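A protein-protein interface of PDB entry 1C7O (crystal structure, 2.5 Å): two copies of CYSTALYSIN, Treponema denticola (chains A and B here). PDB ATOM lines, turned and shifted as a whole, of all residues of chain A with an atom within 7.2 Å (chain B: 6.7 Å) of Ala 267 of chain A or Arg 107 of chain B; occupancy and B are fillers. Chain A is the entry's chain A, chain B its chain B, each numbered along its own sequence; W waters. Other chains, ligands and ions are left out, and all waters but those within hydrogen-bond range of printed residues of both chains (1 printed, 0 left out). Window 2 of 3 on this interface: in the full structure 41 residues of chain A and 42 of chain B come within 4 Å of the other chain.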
ATOM      1  N   ASN A 104      -4.306 -24.055  33.204  1.00  0.00           N
ATOM      2  CA  ASN A 104      -3.517 -22.849  33.069  1.00  0.00           C
ATOM      3  C   ASN A 104      -3.099 -22.296  34.429  1.00  0.00           C
ATOM      4  O   ASN A 104      -2.024 -21.703  34.567  1.00  0.00           O
ATOM      5  CB  ASN A 104      -4.299 -21.802  32.280  1.00  0.00           C
ATOM      6  CG  ASN A 104      -3.425 -20.667  31.821  1.00  0.00           C
ATOM      7  OD1 ASN A 104      -2.468 -20.870  31.065  1.00  0.00           O
ATOM      8  ND2 ASN A 104      -3.733 -19.462  32.282  1.00  0.00           N
ATOM      9  N   ARG A 107      -0.137 -24.482  35.615  1.00  0.00           N
ATOM     10  CA  ARG A 107       1.005 -24.131  34.782  1.00  0.00           C
ATOM     11  C   ARG A 107       1.688 -22.816  35.126  1.00  0.00           C
ATOM     12  O   ARG A 107       2.914 -22.729  35.110  1.00  0.00           O
ATOM     13  CB  ARG A 107       0.573 -24.126  33.308  1.00  0.00           C
ATOM     14  CG  ARG A 107       1.574 -23.501  32.349  1.00  0.00           C
ATOM     15  CD  ARG A 107       1.331 -23.928  30.899  1.00  0.00           C
ATOM     16  NE  ARG A 107      -0.051 -23.751  30.447  1.00  0.00           N
ATOM     17  CZ  ARG A 107      -0.975 -24.714  30.427  1.00  0.00           C
ATOM     18  NH1 ARG A 107      -0.677 -25.943  30.837  1.00  0.00           N
ATOM     19  NH2 ARG A 107      -2.199 -24.446  29.984  1.00  0.00           N
ATOM     20  N   PHE A 261      -2.100 -14.877  34.755  1.00  0.00           N
ATOM     21  CA  PHE A 261      -3.039 -15.848  34.213  1.00  0.00           C
ATOM     22  C   PHE A 261      -3.223 -15.614  32.721  1.00  0.00           C
ATOM     23  O   PHE A 261      -3.194 -16.549  31.928  1.00  0.00           O
ATOM     24  CB  PHE A 261      -4.396 -15.716  34.892  1.00  0.00           C
ATOM     25  CG  PHE A 261      -5.430 -16.661  34.353  1.00  0.00           C
ATOM     26  CD1 PHE A 261      -5.476 -17.983  34.788  1.00  0.00           C
ATOM     27  CD2 PHE A 261      -6.340 -16.238  33.389  1.00  0.00           C
ATOM     28  CE1 PHE A 261      -6.417 -18.872  34.270  1.00  0.00           C
ATOM     29  CE2 PHE A 261      -7.284 -17.119  32.864  1.00  0.00           C
ATOM     30  CZ  PHE A 261      -7.323 -18.441  33.306  1.00  0.00           C
ATOM     31  N   THR A 262      -3.416 -14.354  32.348  1.00  0.00           N
ATOM     32  CA  THR A 262      -3.620 -13.999  30.955  1.00  0.00           C
ATOM     33  C   THR A 262      -2.396 -14.323  30.113  1.00  0.00           C
ATOM     34  O   THR A 262      -2.515 -14.987  29.080  1.00  0.00           O
ATOM     35  CB  THR A 262      -3.953 -12.498  30.793  1.00  0.00           C
ATOM     36  OG1 THR A 262      -5.131 -12.181  31.547  1.00  0.00           O
ATOM     37  CG2 THR A 262      -4.197 -12.162  29.338  1.00  0.00           C
ATOM     38  N   LYS A 263      -1.217 -13.879  30.543  1.00  0.00           N
ATOM     39  CA  LYS A 263      -0.016 -14.151  29.763  1.00  0.00           C
ATOM     40  C   LYS A 263       0.169 -15.654  29.597  1.00  0.00           C
ATOM     41  O   LYS A 263       0.607 -16.120  28.546  1.00  0.00           O
ATOM     42  CB  LYS A 263       1.232 -13.542  30.416  1.00  0.00           C
ATOM     43  CG  LYS A 263       1.883 -14.396  31.485  1.00  0.00           C
ATOM     44  CD  LYS A 263       3.306 -13.932  31.781  1.00  0.00           C
ATOM     45  CE  LYS A 263       3.874 -14.685  32.967  1.00  0.00           C
ATOM     46  NZ  LYS A 263       5.201 -14.166  33.365  1.00  0.00           N
ATOM     47  N   SER A 264      -0.176 -16.407  30.638  1.00  0.00           N
ATOM     48  CA  SER A 264      -0.051 -17.853  30.599  1.00  0.00           C
ATOM     49  C   SER A 264      -1.057 -18.431  29.606  1.00  0.00           C
ATOM     50  O   SER A 264      -0.720 -19.315  28.811  1.00  0.00           O
ATOM     51  CB  SER A 264      -0.286 -18.438  31.992  1.00  0.00           C
ATOM     52  OG  SER A 264      -0.231 -19.856  31.967  1.00  0.00           O
ATOM     53  N   ARG A 265      -2.290 -17.930  29.655  1.00  0.00           N
ATOM     54  CA  ARG A 265      -3.330 -18.388  28.745  1.00  0.00           C
ATOM     55  C   ARG A 265      -2.966 -18.094  27.296  1.00  0.00           C
ATOM     56  O   ARG A 265      -3.351 -18.844  26.394  1.00  0.00           O
ATOM     57  CB  ARG A 265      -4.656 -17.699  29.034  1.00  0.00           C
ATOM     58  CG  ARG A 265      -5.725 -18.033  28.000  1.00  0.00           C
ATOM     59  CD  ARG A 265      -6.753 -16.938  27.887  1.00  0.00           C
ATOM     60  NE  ARG A 265      -6.139 -15.678  27.503  1.00  0.00           N
ATOM     61  CZ  ARG A 265      -6.816 -14.554  27.300  1.00  0.00           C
ATOM     62  NH1 ARG A 265      -8.134 -14.537  27.446  1.00  0.00           N
ATOM     63  NH2 ARG A 265      -6.175 -13.448  26.950  1.00  0.00           N
ATOM     64  N   ASP A 266      -2.244 -16.999  27.072  1.00  0.00           N
ATOM     65  CA  ASP A 266      -1.858 -16.621  25.716  1.00  0.00           C
ATOM     66  C   ASP A 266      -0.675 -17.410  25.176  1.00  0.00           C
ATOM     67  O   ASP A 266      -0.390 -17.365  23.980  1.00  0.00           O
ATOM     68  CB  ASP A 266      -1.551 -15.121  25.628  1.00  0.00           C
ATOM     69  CG  ASP A 266      -2.789 -14.268  25.787  1.00  0.00           C
ATOM     70  OD1 ASP A 266      -3.903 -14.787  25.566  1.00  0.00           O
ATOM     71  OD2 ASP A 266      -2.645 -13.073  26.119  1.00  0.00           O
ATOM     72  N   ALA A 267       0.012 -18.130  26.058  1.00  0.00           N
ATOM     73  CA  ALA A 267       1.152 -18.935  25.641  1.00  0.00           C
ATOM     74  C   ALA A 267       0.681 -20.352  25.344  1.00  0.00           C
ATOM     75  O   ALA A 267       1.439 -21.163  24.829  1.00  0.00           O
ATOM     76  CB  ALA A 267       2.229 -18.942  26.727  1.00  0.00           C
ATOM     77  N   THR A 268      -0.575 -20.649  25.667  1.00  0.00           N
ATOM     78  CA  THR A 268      -1.137 -21.977  25.421  1.00  0.00           C
ATOM     79  C   THR A 268      -2.343 -21.945  24.468  1.00  0.00           C
ATOM     80  O   THR A 268      -2.209 -22.185  23.267  1.00  0.00           O
ATOM     81  CB  THR A 268      -1.570 -22.673  26.746  1.00  0.00           C
ATOM     82  OG1 THR A 268      -2.650 -21.953  27.350  1.00  0.00           O
ATOM     83  CG2 THR A 268      -0.410 -22.722  27.721  1.00  0.00           C
ATOM     84  N   SER A 269      -3.519 -21.645  24.998  1.00  0.00           N
ATOM     85  CA  SER A 269      -4.708 -21.610  24.168  1.00  0.00           C
ATOM     86  C   SER A 269      -4.979 -20.268  23.496  1.00  0.00           C
ATOM     87  O   SER A 269      -5.549 -20.219  22.406  1.00  0.00           O
ATOM     88  CB  SER A 269      -5.917 -22.030  24.995  1.00  0.00           C
ATOM     89  OG  SER A 269      -5.929 -21.348  26.229  1.00  0.00           O
ATOM     90  N   GLY A 270      -4.574 -19.178  24.135  1.00  0.00           N
ATOM     91  CA  GLY A 270      -4.813 -17.866  23.558  1.00  0.00           C
ATOM     92  C   GLY A 270      -6.221 -17.364  23.840  1.00  0.00           C
ATOM     93  O   GLY A 270      -7.039 -18.082  24.418  1.00  0.00           O
ATOM     94  N   PRO B 100      -2.730 -21.494  18.215  1.00  0.00           N
ATOM     95  CA  PRO B 100      -2.592 -22.343  19.403  1.00  0.00           C
ATOM     96  C   PRO B 100      -1.958 -23.677  19.022  1.00  0.00           C
ATOM     97  O   PRO B 100      -1.187 -24.254  19.794  1.00  0.00           O
ATOM     98  CB  PRO B 100      -4.032 -22.499  19.883  1.00  0.00           C
ATOM     99  CG  PRO B 100      -4.645 -21.193  19.492  1.00  0.00           C
ATOM    100  CD  PRO B 100      -4.102 -20.966  18.106  1.00  0.00           C
ATOM    101  N   VAL B 102       0.220 -24.107  16.719  1.00  0.00           N
ATOM    102  CA  VAL B 102       1.645 -23.901  16.497  1.00  0.00           C
ATOM    103  C   VAL B 102       2.390 -23.827  17.826  1.00  0.00           C
ATOM    104  O   VAL B 102       3.512 -24.330  17.948  1.00  0.00           O
ATOM    105  CB  VAL B 102       1.913 -22.619  15.706  1.00  0.00           C
ATOM    106  CG1 VAL B 102       3.399 -22.465  15.471  1.00  0.00           C
ATOM    107  CG2 VAL B 102       1.182 -22.667  14.381  1.00  0.00           C
ATOM    108  N   PHE B 103       1.766 -23.182  18.812  1.00  0.00           N
ATOM    109  CA  PHE B 103       2.350 -23.064  20.148  1.00  0.00           C
ATOM    110  C   PHE B 103       2.477 -24.477  20.695  1.00  0.00           C
ATOM    111  O   PHE B 103       3.508 -24.859  21.247  1.00  0.00           O
ATOM    112  CB  PHE B 103       1.433 -22.267  21.094  1.00  0.00           C
ATOM    113  CG  PHE B 103       1.664 -20.775  21.083  1.00  0.00           C
ATOM    114  CD1 PHE B 103       1.277 -19.997  19.995  1.00  0.00           C
ATOM    115  CD2 PHE B 103       2.224 -20.142  22.197  1.00  0.00           C
ATOM    116  CE1 PHE B 103       1.434 -18.607  20.017  1.00  0.00           C
ATOM    117  CE2 PHE B 103       2.387 -18.755  22.231  1.00  0.00           C
ATOM    118  CZ  PHE B 103       1.985 -17.984  21.132  1.00  0.00           C
ATOM    119  N   ASN B 104       1.415 -25.250  20.526  1.00  0.00           N
ATOM    120  CA  ASN B 104       1.384 -26.611  21.010  1.00  0.00           C
ATOM    121  C   ASN B 104       2.498 -27.436  20.383  1.00  0.00           C
ATOM    122  O   ASN B 104       3.036 -28.344  21.017  1.00  0.00           O
ATOM    123  CB  ASN B 104       0.032 -27.237  20.703  1.00  0.00           C
ATOM    124  CG  ASN B 104      -0.174 -28.546  21.440  1.00  0.00           C
ATOM    125  OD1 ASN B 104      -0.125 -28.592  22.671  1.00  0.00           O
ATOM    126  ND2 ASN B 104      -0.403 -29.622  20.689  1.00  0.00           N
ATOM    127  N   ALA B 105       2.841 -27.110  19.141  1.00  0.00           N
ATOM    128  CA  ALA B 105       3.892 -27.803  18.407  1.00  0.00           C
ATOM    129  C   ALA B 105       5.261 -27.508  19.016  1.00  0.00           C
ATOM    130  O   ALA B 105       6.085 -28.412  19.191  1.00  0.00           O
ATOM    131  CB  ALA B 105       3.869 -27.385  16.949  1.00  0.00           C
ATOM    132  N   VAL B 106       5.500 -26.240  19.337  1.00  0.00           N
ATOM    133  CA  VAL B 106       6.767 -25.837  19.935  1.00  0.00           C
ATOM    134  C   VAL B 106       6.927 -26.585  21.260  1.00  0.00           C
ATOM    135  O   VAL B 106       7.916 -27.290  21.493  1.00  0.00           O
ATOM    136  CB  VAL B 106       6.789 -24.309  20.199  1.00  0.00           C
ATOM    137  CG1 VAL B 106       8.037 -23.923  20.993  1.00  0.00           C
ATOM    138  CG2 VAL B 106       6.742 -23.547  18.867  1.00  0.00           C
ATOM    139  N   ARG B 107       5.914 -26.441  22.105  1.00  0.00           N
ATOM    140  CA  ARG B 107       5.872 -27.052  23.417  1.00  0.00           C
ATOM    141  C   ARG B 107       6.187 -28.548  23.434  1.00  0.00           C
ATOM    142  O   ARG B 107       7.016 -29.003  24.218  1.00  0.00           O
ATOM    143  CB  ARG B 107       4.489 -26.778  24.033  1.00  0.00           C
ATOM    144  CG  ARG B 107       4.181 -27.509  25.337  1.00  0.00           C
ATOM    145  CD  ARG B 107       3.043 -26.819  26.121  1.00  0.00           C
ATOM    146  NE  ARG B 107       1.922 -26.394  25.273  1.00  0.00           N
ATOM    147  CZ  ARG B 107       1.693 -25.138  24.878  1.00  0.00           C
ATOM    148  NH1 ARG B 107       2.505 -24.152  25.253  1.00  0.00           N
ATOM    149  NH2 ARG B 107       0.648 -24.865  24.098  1.00  0.00           N
ATOM    150  N   GLU B 108       5.540 -29.304  22.555  1.00  0.00           N
ATOM    151  CA  GLU B 108       5.717 -30.749  22.512  1.00  0.00           C
ATOM    152  C   GLU B 108       6.959 -31.273  21.816  1.00  0.00           C
ATOM    153  O   GLU B 108       7.590 -32.207  22.307  1.00  0.00           O
ATOM    154  CB  GLU B 108       4.491 -31.400  21.874  1.00  0.00           C
ATOM    155  CG  GLU B 108       4.608 -32.903  21.648  1.00  0.00           C
ATOM    156  CD  GLU B 108       4.797 -33.680  22.940  1.00  0.00           C
ATOM    157  OE1 GLU B 108       4.258 -33.238  23.976  1.00  0.00           O
ATOM    158  OE2 GLU B 108       5.466 -34.741  22.913  1.00  0.00           O
ATOM    159  N   PHE B 109       7.320 -30.675  20.686  1.00  0.00           N
ATOM    160  CA  PHE B 109       8.468 -31.174  19.945  1.00  0.00           C
ATOM    161  C   PHE B 109       9.810 -30.476  20.104  1.00  0.00           C
ATOM    162  O   PHE B 109      10.750 -30.774  19.376  1.00  0.00           O
ATOM    163  CB  PHE B 109       8.101 -31.281  18.466  1.00  0.00           C
ATOM    164  CG  PHE B 109       6.902 -32.149  18.219  1.00  0.00           C
ATOM    165  CD1 PHE B 109       5.637 -31.585  18.045  1.00  0.00           C
ATOM    166  CD2 PHE B 109       7.023 -33.538  18.226  1.00  0.00           C
ATOM    167  CE1 PHE B 109       4.509 -32.393  17.886  1.00  0.00           C
ATOM    168  CE2 PHE B 109       5.893 -34.352  18.066  1.00  0.00           C
ATOM    169  CZ  PHE B 109       4.639 -33.776  17.898  1.00  0.00           C
ATOM    170  N   THR B 110       9.909 -29.544  21.039  1.00  0.00           N
ATOM    171  CA  THR B 110      11.181 -28.873  21.283  1.00  0.00           C
ATOM    172  C   THR B 110      11.204 -28.562  22.765  1.00  0.00           C
ATOM    173  O   THR B 110      10.198 -28.729  23.450  1.00  0.00           O
ATOM    174  CB  THR B 110      11.336 -27.541  20.493  1.00  0.00           C
ATOM    175  OG1 THR B 110      10.567 -26.511  21.123  1.00  0.00           O
ATOM    176  CG2 THR B 110      10.874 -27.708  19.057  1.00  0.00           C
ATOM    177  N   LYS B 111      12.349 -28.121  23.263  1.00  0.00           N
ATOM    178  CA  LYS B 111      12.468 -27.777  24.673  1.00  0.00           C
ATOM    179  C   LYS B 111      13.080 -26.388  24.779  1.00  0.00           C
ATOM    180  O   LYS B 111      13.449 -25.794  23.771  1.00  0.00           O
ATOM    181  CB  LYS B 111      13.354 -28.796  25.397  1.00  0.00           C
ATOM    182  CG  LYS B 111      14.755 -28.849  24.865  1.00  0.00           C
ATOM    183  CD  LYS B 111      15.663 -29.644  25.779  1.00  0.00           C
ATOM    184  CE  LYS B 111      17.079 -29.622  25.237  1.00  0.00           C
ATOM    185  NZ  LYS B 111      17.463 -28.216  24.888  1.00  0.00           N
ATOM    186  N   ALA B 129       5.243 -17.610  19.476  1.00  0.00           N
ATOM    187  CA  ALA B 129       5.150 -19.047  19.692  1.00  0.00           C
ATOM    188  C   ALA B 129       6.499 -19.595  20.115  1.00  0.00           C
ATOM    189  O   ALA B 129       6.580 -20.486  20.957  1.00  0.00           O
ATOM    190  CB  ALA B 129       4.694 -19.734  18.420  1.00  0.00           C
ATOM    191  N   ASN B 132       8.242 -16.659  23.362  1.00  0.00           N
ATOM    192  CA  ASN B 132       7.452 -16.631  24.594  1.00  0.00           C
ATOM    193  C   ASN B 132       7.480 -17.959  25.351  1.00  0.00           C
ATOM    194  O   ASN B 132       6.875 -18.080  26.415  1.00  0.00           O
ATOM    195  CB  ASN B 132       5.998 -16.219  24.318  1.00  0.00           C
ATOM    196  CG  ASN B 132       5.858 -14.730  24.015  1.00  0.00           C
ATOM    197  OD1 ASN B 132       6.830 -13.970  24.098  1.00  0.00           O
ATOM    198  ND2 ASN B 132       4.644 -14.305  23.665  1.00  0.00           N
ATOM    199  N   GLN B 133       8.180 -18.951  24.809  1.00  0.00           N
ATOM    200  CA  GLN B 133       8.284 -20.246  25.465  1.00  0.00           C
ATOM    201  C   GLN B 133       9.742 -20.661  25.658  1.00  0.00           C
ATOM    202  O   GLN B 133      10.056 -21.852  25.696  1.00  0.00           O
ATOM    203  CB  GLN B 133       7.548 -21.331  24.670  1.00  0.00           C
ATOM    204  CG  GLN B 133       6.055 -21.089  24.481  1.00  0.00           C
ATOM    205  CD  GLN B 133       5.331 -22.313  23.932  1.00  0.00           C
ATOM    206  OE1 GLN B 133       5.106 -23.288  24.651  1.00  0.00           O
ATOM    207  NE2 GLN B 133       4.975 -22.271  22.652  1.00  0.00           N
ATOM    208  N   ARG B 135      12.149 -20.705  23.678  1.00  0.00           N
ATOM    209  CA  ARG B 135      12.820 -21.341  22.552  1.00  0.00           C
ATOM    210  C   ARG B 135      13.493 -20.234  21.758  1.00  0.00           C
ATOM    211  O   ARG B 135      13.066 -19.081  21.821  1.00  0.00           O
ATOM    212  CB  ARG B 135      11.826 -22.113  21.676  1.00  0.00           C
ATOM    213  CG  ARG B 135      11.543 -23.541  22.127  1.00  0.00           C
ATOM    214  CD  ARG B 135      10.817 -23.615  23.460  1.00  0.00           C
ATOM    215  NE  ARG B 135      10.331 -24.964  23.744  1.00  0.00           N
ATOM    216  CZ  ARG B 135       9.608 -25.295  24.813  1.00  0.00           C
ATOM    217  NH1 ARG B 135       9.284 -24.374  25.714  1.00  0.00           N
ATOM    218  NH2 ARG B 135       9.191 -26.543  24.975  1.00  0.00           N
ATOM    219  N   TRP B 201       6.777 -27.780  10.078  1.00  0.00           N
ATOM    220  CA  TRP B 201       5.499 -27.288  10.578  1.00  0.00           C
ATOM    221  C   TRP B 201       5.075 -26.315   9.482  1.00  0.00           C
ATOM    222  O   TRP B 201       5.627 -25.224   9.360  1.00  0.00           O
ATOM    223  CB  TRP B 201       5.664 -26.559  11.918  1.00  0.00           C
ATOM    224  CG  TRP B 201       6.294 -27.395  13.021  1.00  0.00           C
ATOM    225  CD1 TRP B 201       6.405 -28.760  13.062  1.00  0.00           C
ATOM    226  CD2 TRP B 201       6.892 -26.911  14.233  1.00  0.00           C
ATOM    227  NE1 TRP B 201       7.038 -29.155  14.220  1.00  0.00           N
ATOM    228  CE2 TRP B 201       7.348 -28.042  14.956  1.00  0.00           C
ATOM    229  CE3 TRP B 201       7.090 -25.631  14.780  1.00  0.00           C
ATOM    230  CZ2 TRP B 201       7.992 -27.931  16.200  1.00  0.00           C
ATOM    231  CZ3 TRP B 201       7.732 -25.520  16.020  1.00  0.00           C
ATOM    232  CH2 TRP B 201       8.174 -26.666  16.713  1.00  0.00           C
ATOM    233  N   SER B 264      -0.275 -33.330  24.119  1.00  0.00           N
ATOM    234  CA  SER B 264       0.184 -32.005  24.489  1.00  0.00           C
ATOM    235  C   SER B 264      -0.982 -31.023  24.414  1.00  0.00           C
ATOM    236  O   SER B 264      -1.070 -30.089  25.206  1.00  0.00           O
ATOM    237  CB  SER B 264       1.292 -31.549  23.553  1.00  0.00           C
ATOM    238  OG  SER B 264       1.708 -30.245  23.907  1.00  0.00           O
ATOM    239  N   ARG B 265      -1.873 -31.248  23.455  1.00  0.00           N
ATOM    240  CA  ARG B 265      -3.036 -30.395  23.269  1.00  0.00           C
ATOM    241  C   ARG B 265      -4.014 -30.574  24.430  1.00  0.00           C
ATOM    242  O   ARG B 265      -4.581 -29.605  24.942  1.00  0.00           O
ATOM    243  CB  ARG B 265      -3.736 -30.745  21.952  1.00  0.00           C
ATOM    244  CG  ARG B 265      -4.910 -29.845  21.618  1.00  0.00           C
ATOM    245  CD  ARG B 265      -5.924 -30.573  20.752  1.00  0.00           C
ATOM    246  NE  ARG B 265      -6.447 -31.756  21.429  1.00  0.00           N
ATOM    247  CZ  ARG B 265      -7.342 -32.580  20.898  1.00  0.00           C
ATOM    248  NH1 ARG B 265      -7.814 -32.339  19.681  1.00  0.00           N
ATOM    249  NH2 ARG B 265      -7.756 -33.652  21.575  1.00  0.00           N
ATOM    250  N   ALA B 267      -3.362 -31.333  27.465  1.00  0.00           N
ATOM    251  CA  ALA B 267      -2.869 -30.870  28.757  1.00  0.00           C
ATOM    252  C   ALA B 267      -2.759 -29.335  28.739  1.00  0.00           C
ATOM    253  O   ALA B 267      -2.342 -28.717  29.723  1.00  0.00           O
ATOM    254  CB  ALA B 267      -1.504 -31.515  29.078  1.00  0.00           C
ATOM    255  N   THR B 268      -3.138 -28.724  27.617  1.00  0.00           N
ATOM    256  CA  THR B 268      -3.085 -27.272  27.490  1.00  0.00           C
ATOM    257  C   THR B 268      -4.447 -26.667  27.152  1.00  0.00           C
ATOM    258  O   THR B 268      -5.127 -26.137  28.027  1.00  0.00           O
ATOM    259  CB  THR B 268      -2.069 -26.843  26.422  1.00  0.00           C
ATOM    260  OG1 THR B 268      -2.365 -27.505  25.187  1.00  0.00           O
ATOM    261  CG2 THR B 268      -0.651 -27.197  26.863  1.00  0.00           C
ATOM    262  N   SER B 269      -4.853 -26.748  25.891  1.00  0.00           N
ATOM    263  CA  SER B 269      -6.137 -26.191  25.489  1.00  0.00           C
ATOM    264  C   SER B 269      -7.268 -27.222  25.506  1.00  0.00           C
ATOM    265  O   SER B 269      -8.442 -26.864  25.603  1.00  0.00           O
ATOM    266  CB  SER B 269      -6.032 -25.580  24.093  1.00  0.00           C
ATOM    267  OG  SER B 269      -5.713 -26.563  23.130  1.00  0.00           O
HETATM  268  O   HOH W   1      -2.023 -25.624  22.977  1.00  0.00           O
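The guanidinium group of Arg 107 of chain A sits at hydrogen-bond distance from the backbone carbonyl oxygen of Ala 267 of chain B, 3.4 Å away.
The backbone carbonyl oxygen (O) of Ala 267 of chain A is in hydrogen-bond range of the guanidinium group (NH1) of Arg 107 of chain B, 3.2 Å away.
OG1 of Thr 268 of chain A sits at hydrogen-bond distance from O of Arg 265 of chain A (3.3 Å).
O of Phe 103 of chain B is in hydrogen-bond range of NE2 of Gln 133 of chain B.
The side-chain amide oxygen (OE1) of Gln 133 of chain B is in hydrogen-bond range of the guanidinium group (NH1) of Arg 107 of chain B (2.8 Å).
The backbone carbonyl oxygen (O) of Arg 107 of chain B sits at hydrogen-bond distance from the guanidinium group (NH2) of Arg 135 of chain B.
The backbone carbonyl oxygen (O) of Ser 264 of chain B lies within hydrogen-bond range of the side-chain hydroxyl (OG1) of Thr 268 of chain B (2.9 Å).
O of Arg 265 of chain B lies within hydrogen-bond range of OG1 of Thr 268 of chain B, 3.1 Å away.
Among the printed residues, pairs that only touch across the chains: Ala 267 of chain A with Phe 103 of chain B (2.9 Å), Ser 269 of chain A with Pro 100 of chain B (3.2 Å), Asp 266 of chain A with Phe 103 of chain B (3.6 Å), Thr 268 of chain A with Arg 107 of chain B (3.6 Å), Ser 269 of chain A with Ser 269 of chain B (3.7 Å), Thr 268 of chain A with Pro 100 of chain B (3.9 Å) and Arg 107 of chain A with Thr 268 of chain B (3.9 Å).
Ala 267 of chain A touches just these residues of chain B: Phe 103 and Arg 107.
Of the printed residues of chain B, Thr 268 of chain A touches Pro 100 and Arg 107.
Printed residues of chain A within 4 Å of Arg 107 of chain B: Ala 267 (3.2 Å) and Thr 268 (3.6 Å).
Of the printed residues of chain A, Thr 268 of chain B touches Arg 107.
Printed residues of chain A within 4 Å of Ser 269 of chain B: Ser 269.
Among the printed residues, 9 pairs touch across the chains.
Arg 107 of chain A touches Ala 267 of chain B, and with the chains exchanged Ala 267 of chain A touches Arg 107 of chain B.
Arg 107 of chain A touches Thr 268 of chain B, and with the chains exchanged Thr 268 of chain A touches Arg 107 of chain B.
Ser 269 of chain A touches its own counterpart, Ser 269 of chain B.
7 positions are printed for both chains.
Water W1 lies within hydrogen-bond range of OG1 of Thr 268 of chain B (2.9 Å), NH2 of Arg 107 of chain B (3.0 Å) and O of Thr 268 of chain A (3.5 Å).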
